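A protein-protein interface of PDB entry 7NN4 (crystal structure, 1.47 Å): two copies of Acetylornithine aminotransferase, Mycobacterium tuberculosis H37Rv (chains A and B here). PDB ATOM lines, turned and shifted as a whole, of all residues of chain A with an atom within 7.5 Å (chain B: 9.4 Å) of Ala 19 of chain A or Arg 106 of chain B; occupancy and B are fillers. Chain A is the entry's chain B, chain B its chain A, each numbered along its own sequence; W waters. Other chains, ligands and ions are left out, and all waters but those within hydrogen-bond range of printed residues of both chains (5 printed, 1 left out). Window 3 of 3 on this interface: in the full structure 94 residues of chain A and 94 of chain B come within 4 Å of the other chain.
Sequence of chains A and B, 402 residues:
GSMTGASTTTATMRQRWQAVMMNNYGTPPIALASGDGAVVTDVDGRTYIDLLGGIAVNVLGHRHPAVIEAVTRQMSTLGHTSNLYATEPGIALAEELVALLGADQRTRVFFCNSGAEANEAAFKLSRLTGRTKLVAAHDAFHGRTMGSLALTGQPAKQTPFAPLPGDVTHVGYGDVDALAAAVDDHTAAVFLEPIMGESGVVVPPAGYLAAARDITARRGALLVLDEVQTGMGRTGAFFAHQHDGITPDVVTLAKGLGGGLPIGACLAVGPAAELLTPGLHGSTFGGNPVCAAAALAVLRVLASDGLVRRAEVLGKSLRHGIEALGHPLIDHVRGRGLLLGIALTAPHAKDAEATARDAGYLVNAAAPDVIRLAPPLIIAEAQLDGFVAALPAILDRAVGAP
Of chain B, only Arg 106 and Arg 108 come within 4 Å of Ala 19 of chain A.
Of chain A, only Ala 19 (2.8 Å) comes within 4 Å of Arg 106 of chain B.
Of the printed residues of chain B, Met 21 of chain A touches Ala 94, Arg 108 and Val 109.
Of the printed residues of chain A, Glu 95 of chain B touches Arg 16 and Val 20.
Printed residues of chain A within 4 Å of Thr 107 of chain B: Val 20 (3.9 Å).
Leu 267 of chain B touches none of the printed residues of chain A.
The nearest residue of chain B that does not touch Ala 19 of chain A is Thr 107 of chain B (4.4 Å).
The side-chain carboxylate (OE2) of Glu 95 of chain B lies within salt-bridge range of the guanidinium group (NE) of Arg 16 of chain A (2.9 Å).
The backbone carbonyl oxygen (O) of Ala 19 of chain A sits at hydrogen-bond distance from the guanidinium group (NH1) of Arg 106 of chain B, at 2.8 Å.
The guanidinium group of Arg 108 of chain B lies within hydrogen-bond range of the backbone carbonyl oxygen of Gln 18 of chain A (2.7 Å).
NH1 of Arg 108 of chain B sits at hydrogen-bond distance from O of Met 21 of chain A (2.9 Å).
The backbone NH of Val 109 of chain B sits at hydrogen-bond distance from the backbone carbonyl oxygen of Val 20 of chain A.
N of Met 22 of chain A sits at hydrogen-bond distance from O of Val 109 of chain B (2.9 Å).
Water W2 bridges OE2 of Glu 95 of chain B (2.7 Å) and O of Arg 16 of chain A (2.9 Å).
Water W5 bridges the backbone carbonyl oxygen (O) of Thr 107 of chain B (2.7 Å) and the backbone carbonyl oxygen (O) of Ala 19 of chain A (2.8 Å).
Water W1 lies within hydrogen-bond range of O of Met 21 of chain A (2.8 Å) and NH1 of Arg 108 of chain B (3.4 Å).
Water W3 bridges O of Val 109 of chain B and O of Met 22 of chain A.
Water W4 bridges the side-chain sulfur (SD) of Met 21 of chain A (3.4 Å) and the backbone NH (N) of Ile 91 of chain B (3.5 Å).
No position is printed for both chains.
Of the 18 pairs that touch across the chains among the printed residues, none has its exchanged pair printed and touching as well.
Of the 10 printed residues of chain A, 7 touch a printed residue of chain B.
Printed residues of chain A that touch a printed residue of chain B: Met 13, Arg 16, Gln 18, Ala 19, Val 20, Met 21 and Met 22.
Hydrophobic or aromatic side chains of chain A that line the printed part of chain B: Met 13, Ala 19, Val 20, Met 21 and Met 22.
Hydrophobic or aromatic side chains of chain B within 4 Å of the printed part of chain A: Ile 91, Ala 94, Val 98, Val 109 and Ala 268.
Among the printed residues, Asp or Glu carboxylates within 4 Å of a Lys or Arg side-chain nitrogen of the other chain: Arg 16 of chain A with Glu 95 of chain B.
The backbone carbonyl oxygen (O) of Gln 105 of chain B is in hydrogen-bond range of the side-chain hydroxyl (OG1) of Thr 107 of chain B.
O of Arg 106 of chain B lies within hydrogen-bond range of N of Gly 270 of chain B (2.8 Å).
The backbone carbonyl oxygen (O) of Ala 268 of chain B sits at hydrogen-bond distance from the backbone NH (N) of Arg 108 of chain B (2.9 Å).
OE2 of Glu 274 of chain B is in salt-bridge range of NE of Arg 108 of chain B.
The side-chain sulfur (SD) of Met 13 of chain A lies within hydrogen-bond range of the guanidinium group (NH1) of Arg 16 of chain A.
Ile 91 of chain B touches Met 13 of chain A.
Arg 16 of chain A touches Ile 91 of chain B.
Arg 108 of chain B touches Ala 19 of chain A (NH1 to C, 3.8 Å).
N of Glu 95 of chain B touches CG2 of Val 20 of chain A, 3.8 Å away.
Val 20 of chain A touches Val 98 of chain B (CG2 to CG2, 3.7 Å).
Thr 107 of chain B touches Val 20 of chain A.
O of Val 20 of chain A touches CA of Arg 108 of chain B, 3.1 Å away.
Met 21 of chain A touches Val 109 of chain B.
O of Arg 108 of chain B touches CE of Met 22 of chain A, 3.6 Å away.
CE of Met 22 of chain A touches CB of Ala 268 of chain B (3.6 Å).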
ATOM      1  N   MET A  13      22.385   9.004  32.155  1.00  0.00           N
ATOM      2  CA  MET A  13      22.677  10.143  31.291  1.00  0.00           C
ATOM      3  C   MET A  13      24.103  10.087  30.763  1.00  0.00           C
ATOM      4  O   MET A  13      24.344  10.365  29.581  1.00  0.00           O
ATOM      5  CB  MET A  13      22.428  11.438  32.058  1.00  0.00           C
ATOM      6  CG  MET A  13      20.982  11.800  32.127  1.00  0.00           C
ATOM      7  SD  MET A  13      20.443  12.455  30.541  1.00  0.00           S
ATOM      8  CE  MET A  13      21.111  14.117  30.721  1.00  0.00           C
ATOM      9  N   ARG A  14      25.063   9.734  31.622  1.00  0.00           N
ATOM     10  CA  ARG A  14      26.448   9.617  31.179  1.00  0.00           C
ATOM     11  C   ARG A  14      26.621   8.499  30.160  1.00  0.00           C
ATOM     12  O   ARG A  14      27.416   8.631  29.221  1.00  0.00           O
ATOM     13  CB  ARG A  14      27.386   9.438  32.378  1.00  0.00           C
ATOM     14  CG  ARG A  14      27.454  10.674  33.288  1.00  0.00           C
ATOM     15  CD  ARG A  14      28.353  10.480  34.513  1.00  0.00           C
ATOM     16  NE  ARG A  14      29.779  10.451  34.182  1.00  0.00           N
ATOM     17  CZ  ARG A  14      30.476   9.338  33.990  1.00  0.00           C
ATOM     18  NH1 ARG A  14      29.880   8.160  34.094  1.00  0.00           N
ATOM     19  NH2 ARG A  14      31.769   9.394  33.692  1.00  0.00           N
ATOM     20  N   GLN A  15      25.836   7.439  30.281  1.00  0.00           N
ATOM     21  CA  GLN A  15      25.962   6.331  29.311  1.00  0.00           C
ATOM     22  C   GLN A  15      25.406   6.800  27.969  1.00  0.00           C
ATOM     23  O   GLN A  15      25.964   6.466  26.978  1.00  0.00           O
ATOM     24  CB  GLN A  15      25.266   5.069  29.814  1.00  0.00           C
ATOM     25  CG  GLN A  15      26.054   4.373  30.907  1.00  0.00           C
ATOM     26  CD  GLN A  15      25.253   3.383  31.719  1.00  0.00           C
ATOM     27  OE1 GLN A  15      24.047   3.265  31.559  1.00  0.00           O
ATOM     28  NE2 GLN A  15      25.918   2.625  32.566  1.00  0.00           N
ATOM     29  N   ARG A  16      24.305   7.513  28.008  1.00  0.00           N
ATOM     30  CA  ARG A  16      23.772   8.071  26.768  1.00  0.00           C
ATOM     31  C   ARG A  16      24.772   9.019  26.119  1.00  0.00           C
ATOM     32  O   ARG A  16      24.983   8.972  24.901  1.00  0.00           O
ATOM     33  CB  ARG A  16      22.443   8.778  27.021  1.00  0.00           C
ATOM     34  CG  ARG A  16      21.277   7.838  27.313  1.00  0.00           C
ATOM     35  CD  ARG A  16      20.054   8.620  27.722  1.00  0.00           C
ATOM     36  NE  ARG A  16      19.568   9.481  26.645  1.00  0.00           N
ATOM     37  CZ  ARG A  16      18.691  10.461  26.812  1.00  0.00           C
ATOM     38  NH1 ARG A  16      18.200  10.719  28.020  1.00  0.00           N
ATOM     39  NH2 ARG A  16      18.299  11.185  25.773  1.00  0.00           N
ATOM     40  N   TRP A  17      25.394   9.891  26.921  1.00  0.00           N
ATOM     41  CA  TRP A  17      26.422  10.777  26.388  1.00  0.00           C
ATOM     42  C   TRP A  17      27.509   9.977  25.684  1.00  0.00           C
ATOM     43  O   TRP A  17      27.866  10.260  24.531  1.00  0.00           O
ATOM     44  CB  TRP A  17      27.011  11.618  27.531  1.00  0.00           C
ATOM     45  CG  TRP A  17      28.213  12.430  27.141  1.00  0.00           C
ATOM     46  CD1 TRP A  17      29.488  11.982  26.948  1.00  0.00           C
ATOM     47  CD2 TRP A  17      28.245  13.845  26.919  1.00  0.00           C
ATOM     48  NE1 TRP A  17      30.312  13.032  26.594  1.00  0.00           N
ATOM     49  CE2 TRP A  17      29.569  14.186  26.576  1.00  0.00           C
ATOM     50  CE3 TRP A  17      27.279  14.855  26.982  1.00  0.00           C
ATOM     51  CZ2 TRP A  17      29.953  15.498  26.280  1.00  0.00           C
ATOM     52  CZ3 TRP A  17      27.657  16.165  26.691  1.00  0.00           C
ATOM     53  CH2 TRP A  17      28.984  16.469  26.343  1.00  0.00           C
ATOM     54  N   GLN A  18      28.029   8.949  26.357  1.00  0.00           N
ATOM     55  CA  GLN A  18      29.136   8.182  25.810  1.00  0.00           C
ATOM     56  C   GLN A  18      28.756   7.405  24.559  1.00  0.00           C
ATOM     57  O   GLN A  18      29.646   7.041  23.785  1.00  0.00           O
ATOM     58  CB  GLN A  18      29.687   7.225  26.869  1.00  0.00           C
ATOM     59  CG  GLN A  18      30.400   7.926  28.002  1.00  0.00           C
ATOM     60  CD  GLN A  18      30.740   6.983  29.137  1.00  0.00           C
ATOM     61  OE1 GLN A  18      29.982   6.060  29.444  1.00  0.00           O
ATOM     62  NE2 GLN A  18      31.886   7.214  29.770  1.00  0.00           N
ATOM     63  N   ALA A  19      27.470   7.143  24.344  1.00  0.00           N
ATOM     64  CA  ALA A  19      27.060   6.390  23.166  1.00  0.00           C
ATOM     65  C   ALA A  19      26.984   7.252  21.913  1.00  0.00           C
ATOM     66  O   ALA A  19      27.024   6.708  20.801  1.00  0.00           O
ATOM     67  CB  ALA A  19      25.704   5.723  23.415  1.00  0.00           C
ATOM     68  N   VAL A  20      26.889   8.576  22.054  1.00  0.00           N
ATOM     69  CA  VAL A  20      26.560   9.418  20.908  1.00  0.00           C
ATOM     70  C   VAL A  20      27.473  10.629  20.751  1.00  0.00           C
ATOM     71  O   VAL A  20      27.673  11.119  19.634  1.00  0.00           O
ATOM     72  CB  VAL A  20      25.076   9.825  20.928  1.00  0.00           C
ATOM     73  CG1 VAL A  20      24.821  10.869  22.005  1.00  0.00           C
ATOM     74  CG2 VAL A  20      24.654  10.353  19.573  1.00  0.00           C
ATOM     75  N   MET A  21      28.028  11.145  21.847  1.00  0.00           N
ATOM     76  CA  MET A  21      28.804  12.374  21.735  1.00  0.00           C
ATOM     77  C   MET A  21      30.241  12.075  21.336  1.00  0.00           C
ATOM     78  O   MET A  21      30.813  11.058  21.731  1.00  0.00           O
ATOM     79  CB  MET A  21      28.795  13.143  23.063  1.00  0.00           C
ATOM     80  CG  MET A  21      27.399  13.532  23.535  1.00  0.00           C
ATOM     81  SD  MET A  21      26.454  14.488  22.331  1.00  0.00           S
ATOM     82  CE  MET A  21      27.561  15.858  21.963  1.00  0.00           C
ATOM     83  N   MET A  22      30.835  12.965  20.543  1.00  0.00           N
ATOM     84  CA  MET A  22      32.277  12.887  20.392  1.00  0.00           C
ATOM     85  C   MET A  22      32.927  13.088  21.753  1.00  0.00           C
ATOM     86  O   MET A  22      32.343  13.690  22.656  1.00  0.00           O
ATOM     87  CB  MET A  22      32.772  13.929  19.402  1.00  0.00           C
ATOM     88  CG  MET A  22      32.530  13.482  17.971  1.00  0.00           C
ATOM     89  SD  MET A  22      33.372  14.577  16.856  1.00  0.00           S
ATOM     90  CE  MET A  22      32.324  14.450  15.420  1.00  0.00           C
ATOM     91  N   ILE B  91      21.990  15.748  24.270  1.00  0.00           N
ATOM     92  CA  ILE B  91      22.124  14.304  24.111  1.00  0.00           C
ATOM     93  C   ILE B  91      21.002  13.765  23.230  1.00  0.00           C
ATOM     94  O   ILE B  91      21.241  12.988  22.298  1.00  0.00           O
ATOM     95  CB  ILE B  91      22.181  13.608  25.483  1.00  0.00           C
ATOM     96  CG1 ILE B  91      23.432  14.050  26.236  1.00  0.00           C
ATOM     97  CG2 ILE B  91      22.152  12.084  25.313  1.00  0.00           C
ATOM     98  CD1 ILE B  91      23.447  13.602  27.708  1.00  0.00           C
ATOM     99  N   ALA B  94      21.539  14.790  19.580  1.00  0.00           N
ATOM    100  CA  ALA B  94      22.571  13.968  18.965  1.00  0.00           C
ATOM    101  C   ALA B  94      22.021  12.593  18.608  1.00  0.00           C
ATOM    102  O   ALA B  94      22.263  12.087  17.508  1.00  0.00           O
ATOM    103  CB  ALA B  94      23.776  13.861  19.902  1.00  0.00           C
ATOM    104  N   GLU B  95      21.251  11.994  19.515  1.00  0.00           N
ATOM    105  CA  GLU B  95      20.633  10.701  19.228  1.00  0.00           C
ATOM    106  C   GLU B  95      19.709  10.792  18.019  1.00  0.00           C
ATOM    107  O   GLU B  95      19.733   9.915  17.142  1.00  0.00           O
ATOM    108  CB  GLU B  95      19.863  10.217  20.459  1.00  0.00           C
ATOM    109  CG  GLU B  95      20.749   9.838  21.656  1.00  0.00           C
ATOM    110  CD  GLU B  95      19.961   9.666  22.956  1.00  0.00           C
ATOM    111  OE1 GLU B  95      18.831  10.182  23.043  1.00  0.00           O
ATOM    112  OE2 GLU B  95      20.494   9.028  23.887  1.00  0.00           O
ATOM    113  N   VAL B  98      21.785  11.207  14.754  1.00  0.00           N
ATOM    114  CA  VAL B  98      22.436   9.957  14.368  1.00  0.00           C
ATOM    115  C   VAL B  98      21.420   9.000  13.743  1.00  0.00           C
ATOM    116  O   VAL B  98      21.704   8.344  12.734  1.00  0.00           O
ATOM    117  CB  VAL B  98      23.170   9.340  15.574  1.00  0.00           C
ATOM    118  CG1 VAL B  98      23.534   7.888  15.311  1.00  0.00           C
ATOM    119  CG2 VAL B  98      24.427  10.147  15.898  1.00  0.00           C
ATOM    120  N   LEU B 101      20.710  10.140  10.157  1.00  0.00           N
ATOM    121  CA  LEU B 101      21.776   9.803   9.223  1.00  0.00           C
ATOM    122  C   LEU B 101      21.726   8.324   8.851  1.00  0.00           C
ATOM    123  O   LEU B 101      21.944   7.963   7.689  1.00  0.00           O
ATOM    124  CB  LEU B 101      23.137  10.174   9.822  1.00  0.00           C
ATOM    125  CG  LEU B 101      24.357  10.022   8.908  1.00  0.00           C
ATOM    126  CD1 LEU B 101      24.233  10.912   7.684  1.00  0.00           C
ATOM    127  CD2 LEU B 101      25.638  10.345   9.670  1.00  0.00           C
ATOM    128  N   GLY B 102      21.447   7.458   9.822  1.00  0.00           N
ATOM    129  CA  GLY B 102      21.251   6.046   9.534  1.00  0.00           C
ATOM    130  C   GLY B 102      22.485   5.333   9.037  1.00  0.00           C
ATOM    131  O   GLY B 102      22.374   4.397   8.235  1.00  0.00           O
ATOM    132  N   ALA B 103      23.663   5.744   9.486  1.00  0.00           N
ATOM    133  CA  ALA B 103      24.878   5.059   9.083  1.00  0.00           C
ATOM    134  C   ALA B 103      24.964   3.701   9.773  1.00  0.00           C
ATOM    135  O   ALA B 103      24.377   3.478  10.835  1.00  0.00           O
ATOM    136  CB  ALA B 103      26.107   5.905   9.422  1.00  0.00           C
ATOM    137  N   ASP B 104      25.709   2.787   9.159  1.00  0.00           N
ATOM    138  CA  ASP B 104      25.818   1.446   9.721  1.00  0.00           C
ATOM    139  C   ASP B 104      26.883   1.339  10.804  1.00  0.00           C
ATOM    140  O   ASP B 104      26.813   0.426  11.634  1.00  0.00           O
ATOM    141  CB  ASP B 104      26.032   0.413   8.611  1.00  0.00           C
ATOM    142  CG  ASP B 104      24.864   0.356   7.642  1.00  0.00           C
ATOM    143  OD1 ASP B 104      23.699   0.390   8.106  1.00  0.00           O
ATOM    144  OD2 ASP B 104      25.106   0.285   6.417  1.00  0.00           O
ATOM    145  N   GLN B 105      27.853   2.249  10.824  1.00  0.00           N
ATOM    146  CA  GLN B 105      28.855   2.303  11.876  1.00  0.00           C
ATOM    147  C   GLN B 105      28.455   3.341  12.916  1.00  0.00           C
ATOM    148  O   GLN B 105      27.567   4.171  12.692  1.00  0.00           O
ATOM    149  CB  GLN B 105      30.225   2.657  11.297  1.00  0.00           C
ATOM    150  CG  GLN B 105      30.690   1.736  10.192  1.00  0.00           C
ATOM    151  CD  GLN B 105      31.789   2.355   9.362  1.00  0.00           C
ATOM    152  OE1 GLN B 105      31.524   3.030   8.367  1.00  0.00           O
ATOM    153  NE2 GLN B 105      33.031   2.134   9.769  1.00  0.00           N
ATOM    154  N   ARG B 106      29.120   3.285  14.066  1.00  0.00           N
ATOM    155  CA  ARG B 106      28.820   4.251  15.110  1.00  0.00           C
ATOM    156  C   ARG B 106      29.123   5.655  14.615  1.00  0.00           C
ATOM    157  O   ARG B 106      30.136   5.899  13.954  1.00  0.00           O
ATOM    158  CB  ARG B 106      29.619   3.977  16.383  1.00  0.00           C
ATOM    159  CG  ARG B 106      29.231   4.956  17.502  1.00  0.00           C
ATOM    160  CD  ARG B 106      29.865   4.624  18.823  1.00  0.00           C
ATOM    161  NE  ARG B 106      29.482   3.297  19.287  1.00  0.00           N
ATOM    162  CZ  ARG B 106      28.395   3.027  20.003  1.00  0.00           C
ATOM    163  NH1 ARG B 106      27.553   3.995  20.358  1.00  0.00           N
ATOM    164  NH2 ARG B 106      28.154   1.776  20.373  1.00  0.00           N
ATOM    165  N   THR B 107      28.221   6.569  14.935  1.00  0.00           N
ATOM    166  CA  THR B 107      28.315   7.967  14.564  1.00  0.00           C
ATOM    167  C   THR B 107      28.335   8.778  15.847  1.00  0.00           C
ATOM    168  O   THR B 107      27.575   8.498  16.775  1.00  0.00           O
ATOM    169  CB  THR B 107      27.080   8.347  13.767  1.00  0.00           C
ATOM    170  OG1 THR B 107      26.927   7.413  12.688  1.00  0.00           O
ATOM    171  CG2 THR B 107      27.209   9.756  13.219  1.00  0.00           C
ATOM    172  N   ARG B 108      29.212   9.780  15.900  1.00  0.00           N
ATOM    173  CA  ARG B 108      29.320  10.644  17.064  1.00  0.00           C
ATOM    174  C   ARG B 108      29.135  12.096  16.642  1.00  0.00           C
ATOM    175  O   ARG B 108      29.362  12.462  15.489  1.00  0.00           O
ATOM    176  CB  ARG B 108      30.651  10.443  17.797  1.00  0.00           C
ATOM    177  CG  ARG B 108      30.790   9.051  18.394  1.00  0.00           C
ATOM    178  CD  ARG B 108      32.065   8.901  19.187  1.00  0.00           C
ATOM    179  NE  ARG B 108      32.128   7.590  19.828  1.00  0.00           N
ATOM    180  CZ  ARG B 108      31.450   7.263  20.924  1.00  0.00           C
ATOM    181  NH1 ARG B 108      30.661   8.157  21.517  1.00  0.00           N
ATOM    182  NH2 ARG B 108      31.560   6.038  21.426  1.00  0.00           N
ATOM    183  N   VAL B 109      28.730  12.928  17.602  1.00  0.00           N
ATOM    184  CA  VAL B 109      28.247  14.274  17.325  1.00  0.00           C
ATOM    185  C   VAL B 109      29.056  15.292  18.114  1.00  0.00           C
ATOM    186  O   VAL B 109      29.370  15.074  19.289  1.00  0.00           O
ATOM    187  CB  VAL B 109      26.757  14.409  17.689  1.00  0.00           C
ATOM    188  CG1 VAL B 109      26.245  15.807  17.355  1.00  0.00           C
ATOM    189  CG2 VAL B 109      25.936  13.346  16.952  1.00  0.00           C
ATOM    190  N   THR B 247      27.269   7.082   2.258  1.00  0.00           N
ATOM    191  CA  THR B 247      27.499   7.513   3.635  1.00  0.00           C
ATOM    192  C   THR B 247      28.853   8.194   3.651  1.00  0.00           C
ATOM    193  O   THR B 247      29.879   7.531   3.412  1.00  0.00           O
ATOM    194  CB  THR B 247      27.503   6.326   4.599  1.00  0.00           C
ATOM    195  OG1 THR B 247      26.227   5.666   4.567  1.00  0.00           O
ATOM    196  CG2 THR B 247      27.797   6.800   6.032  1.00  0.00           C
ATOM    197  N   PRO B 248      28.918   9.491   3.902  1.00  0.00           N
ATOM    198  CA  PRO B 248      30.215  10.153   4.037  1.00  0.00           C
ATOM    199  C   PRO B 248      30.834   9.822   5.386  1.00  0.00           C
ATOM    200  O   PRO B 248      30.226   9.187   6.244  1.00  0.00           O
ATOM    201  CB  PRO B 248      29.855  11.633   3.957  1.00  0.00           C
ATOM    202  CG  PRO B 248      28.491  11.682   4.531  1.00  0.00           C
ATOM    203  CD  PRO B 248      27.797  10.413   4.151  1.00  0.00           C
ATOM    204  N   ASP B 249      32.085  10.235   5.546  1.00  0.00           N
ATOM    205  CA  ASP B 249      32.736  10.075   6.840  1.00  0.00           C
ATOM    206  C   ASP B 249      32.329  11.167   7.813  1.00  0.00           C
ATOM    207  O   ASP B 249      32.265  10.916   9.022  1.00  0.00           O
ATOM    208  CB  ASP B 249      34.245  10.091   6.650  1.00  0.00           C
ATOM    209  CG  ASP B 249      34.692   9.031   5.668  1.00  0.00           C
ATOM    210  OD1 ASP B 249      34.456   7.844   5.964  1.00  0.00           O
ATOM    211  OD2 ASP B 249      35.232   9.392   4.607  1.00  0.00           O
ATOM    212  N   LEU B 267      28.850  15.676  12.481  1.00  0.00           N
ATOM    213  CA  LEU B 267      28.639  14.252  12.691  1.00  0.00           C
ATOM    214  C   LEU B 267      29.768  13.511  11.993  1.00  0.00           C
ATOM    215  O   LEU B 267      30.108  13.827  10.846  1.00  0.00           O
ATOM    216  CB  LEU B 267      27.300  13.801  12.099  1.00  0.00           C
ATOM    217  CG  LEU B 267      26.068  13.926  13.008  1.00  0.00           C
ATOM    218  CD1 LEU B 267      25.748  15.357  13.325  1.00  0.00           C
ATOM    219  CD2 LEU B 267      24.860  13.204  12.414  1.00  0.00           C
ATOM    220  N   ALA B 268      30.353  12.536  12.679  1.00  0.00           N
ATOM    221  CA  ALA B 268      31.415  11.733  12.091  1.00  0.00           C
ATOM    222  C   ALA B 268      31.099  10.256  12.272  1.00  0.00           C
ATOM    223  O   ALA B 268      30.576   9.840  13.310  1.00  0.00           O
ATOM    224  CB  ALA B 268      32.777  12.069  12.701  1.00  0.00           C
ATOM    225  N   VAL B 269      31.447   9.464  11.260  1.00  0.00           N
ATOM    226  CA  VAL B 269      31.009   8.081  11.146  1.00  0.00           C
ATOM    227  C   VAL B 269      32.229   7.175  11.203  1.00  0.00           C
ATOM    228  O   VAL B 269      33.242   7.451  10.550  1.00  0.00           O
ATOM    229  CB  VAL B 269      30.232   7.869   9.836  1.00  0.00           C
ATOM    230  CG1 VAL B 269      29.855   6.396   9.659  1.00  0.00           C
ATOM    231  CG2 VAL B 269      29.001   8.761   9.816  1.00  0.00           C
ATOM    232  N   GLY B 270      32.130   6.104  11.992  1.00  0.00           N
ATOM    233  CA  GLY B 270      33.159   5.094  12.046  1.00  0.00           C
ATOM    234  C   GLY B 270      34.434   5.593  12.693  1.00  0.00           C
ATOM    235  O   GLY B 270      34.405   6.297  13.708  1.00  0.00           O
ATOM    236  N   PRO B 271      35.582   5.235  12.112  1.00  0.00           N
ATOM    237  CA  PRO B 271      36.862   5.685  12.684  1.00  0.00           C
ATOM    238  C   PRO B 271      36.960   7.191  12.839  1.00  0.00           C
ATOM    239  O   PRO B 271      37.584   7.662  13.799  1.00  0.00           O
ATOM    240  CB  PRO B 271      37.898   5.149  11.686  1.00  0.00           C
ATOM    241  CG  PRO B 271      37.216   3.987  11.032  1.00  0.00           C
ATOM    242  CD  PRO B 271      35.775   4.362  10.938  1.00  0.00           C
ATOM    243  N   ALA B 272      36.344   7.961  11.937  1.00  0.00           N
ATOM    244  CA  ALA B 272      36.408   9.414  12.049  1.00  0.00           C
ATOM    245  C   ALA B 272      35.753   9.905  13.337  1.00  0.00           C
ATOM    246  O   ALA B 272      36.126  10.966  13.859  1.00  0.00           O
ATOM    247  CB  ALA B 272      35.762  10.071  10.827  1.00  0.00           C
ATOM    248  N   ALA B 273      34.793   9.144  13.871  1.00  0.00           N
ATOM    249  CA  ALA B 273      34.084   9.540  15.083  1.00  0.00           C
ATOM    250  C   ALA B 273      34.962   9.459  16.322  1.00  0.00           C
ATOM    251  O   ALA B 273      34.608  10.041  17.352  1.00  0.00           O
ATOM    252  CB  ALA B 273      32.850   8.657  15.284  1.00  0.00           C
ATOM    253  N   GLU B 274      36.089   8.758  16.252  1.00  0.00           N
ATOM    254  CA  GLU B 274      36.957   8.560  17.406  1.00  0.00           C
ATOM    255  C   GLU B 274      38.188   9.455  17.386  1.00  0.00           C
ATOM    256  O   GLU B 274      38.980   9.420  18.336  1.00  0.00           O
ATOM    257  CB  GLU B 274      37.379   7.086  17.501  1.00  0.00           C
ATOM    258  CG  GLU B 274      36.219   6.105  17.326  1.00  0.00           C
ATOM    259  CD  GLU B 274      35.169   6.245  18.413  1.00  0.00           C
ATOM    260  OE1 GLU B 274      35.553   6.409  19.593  1.00  0.00           O
ATOM    261  OE2 GLU B 274      33.959   6.194  18.101  1.00  0.00           O
HETATM  262  O   HOH W   1      31.653   9.995  24.200  1.00  0.00           O
HETATM  263  O   HOH W   2      22.801   7.748  23.499  1.00  0.00           O
HETATM  264  O   HOH W   3      31.035  16.648  21.712  1.00  0.00           O
HETATM  265  O   HOH W   4      25.164  17.147  24.064  1.00  0.00           O
HETATM  266  O   HOH W   5      25.806   7.001  18.245  1.00  0.00           O
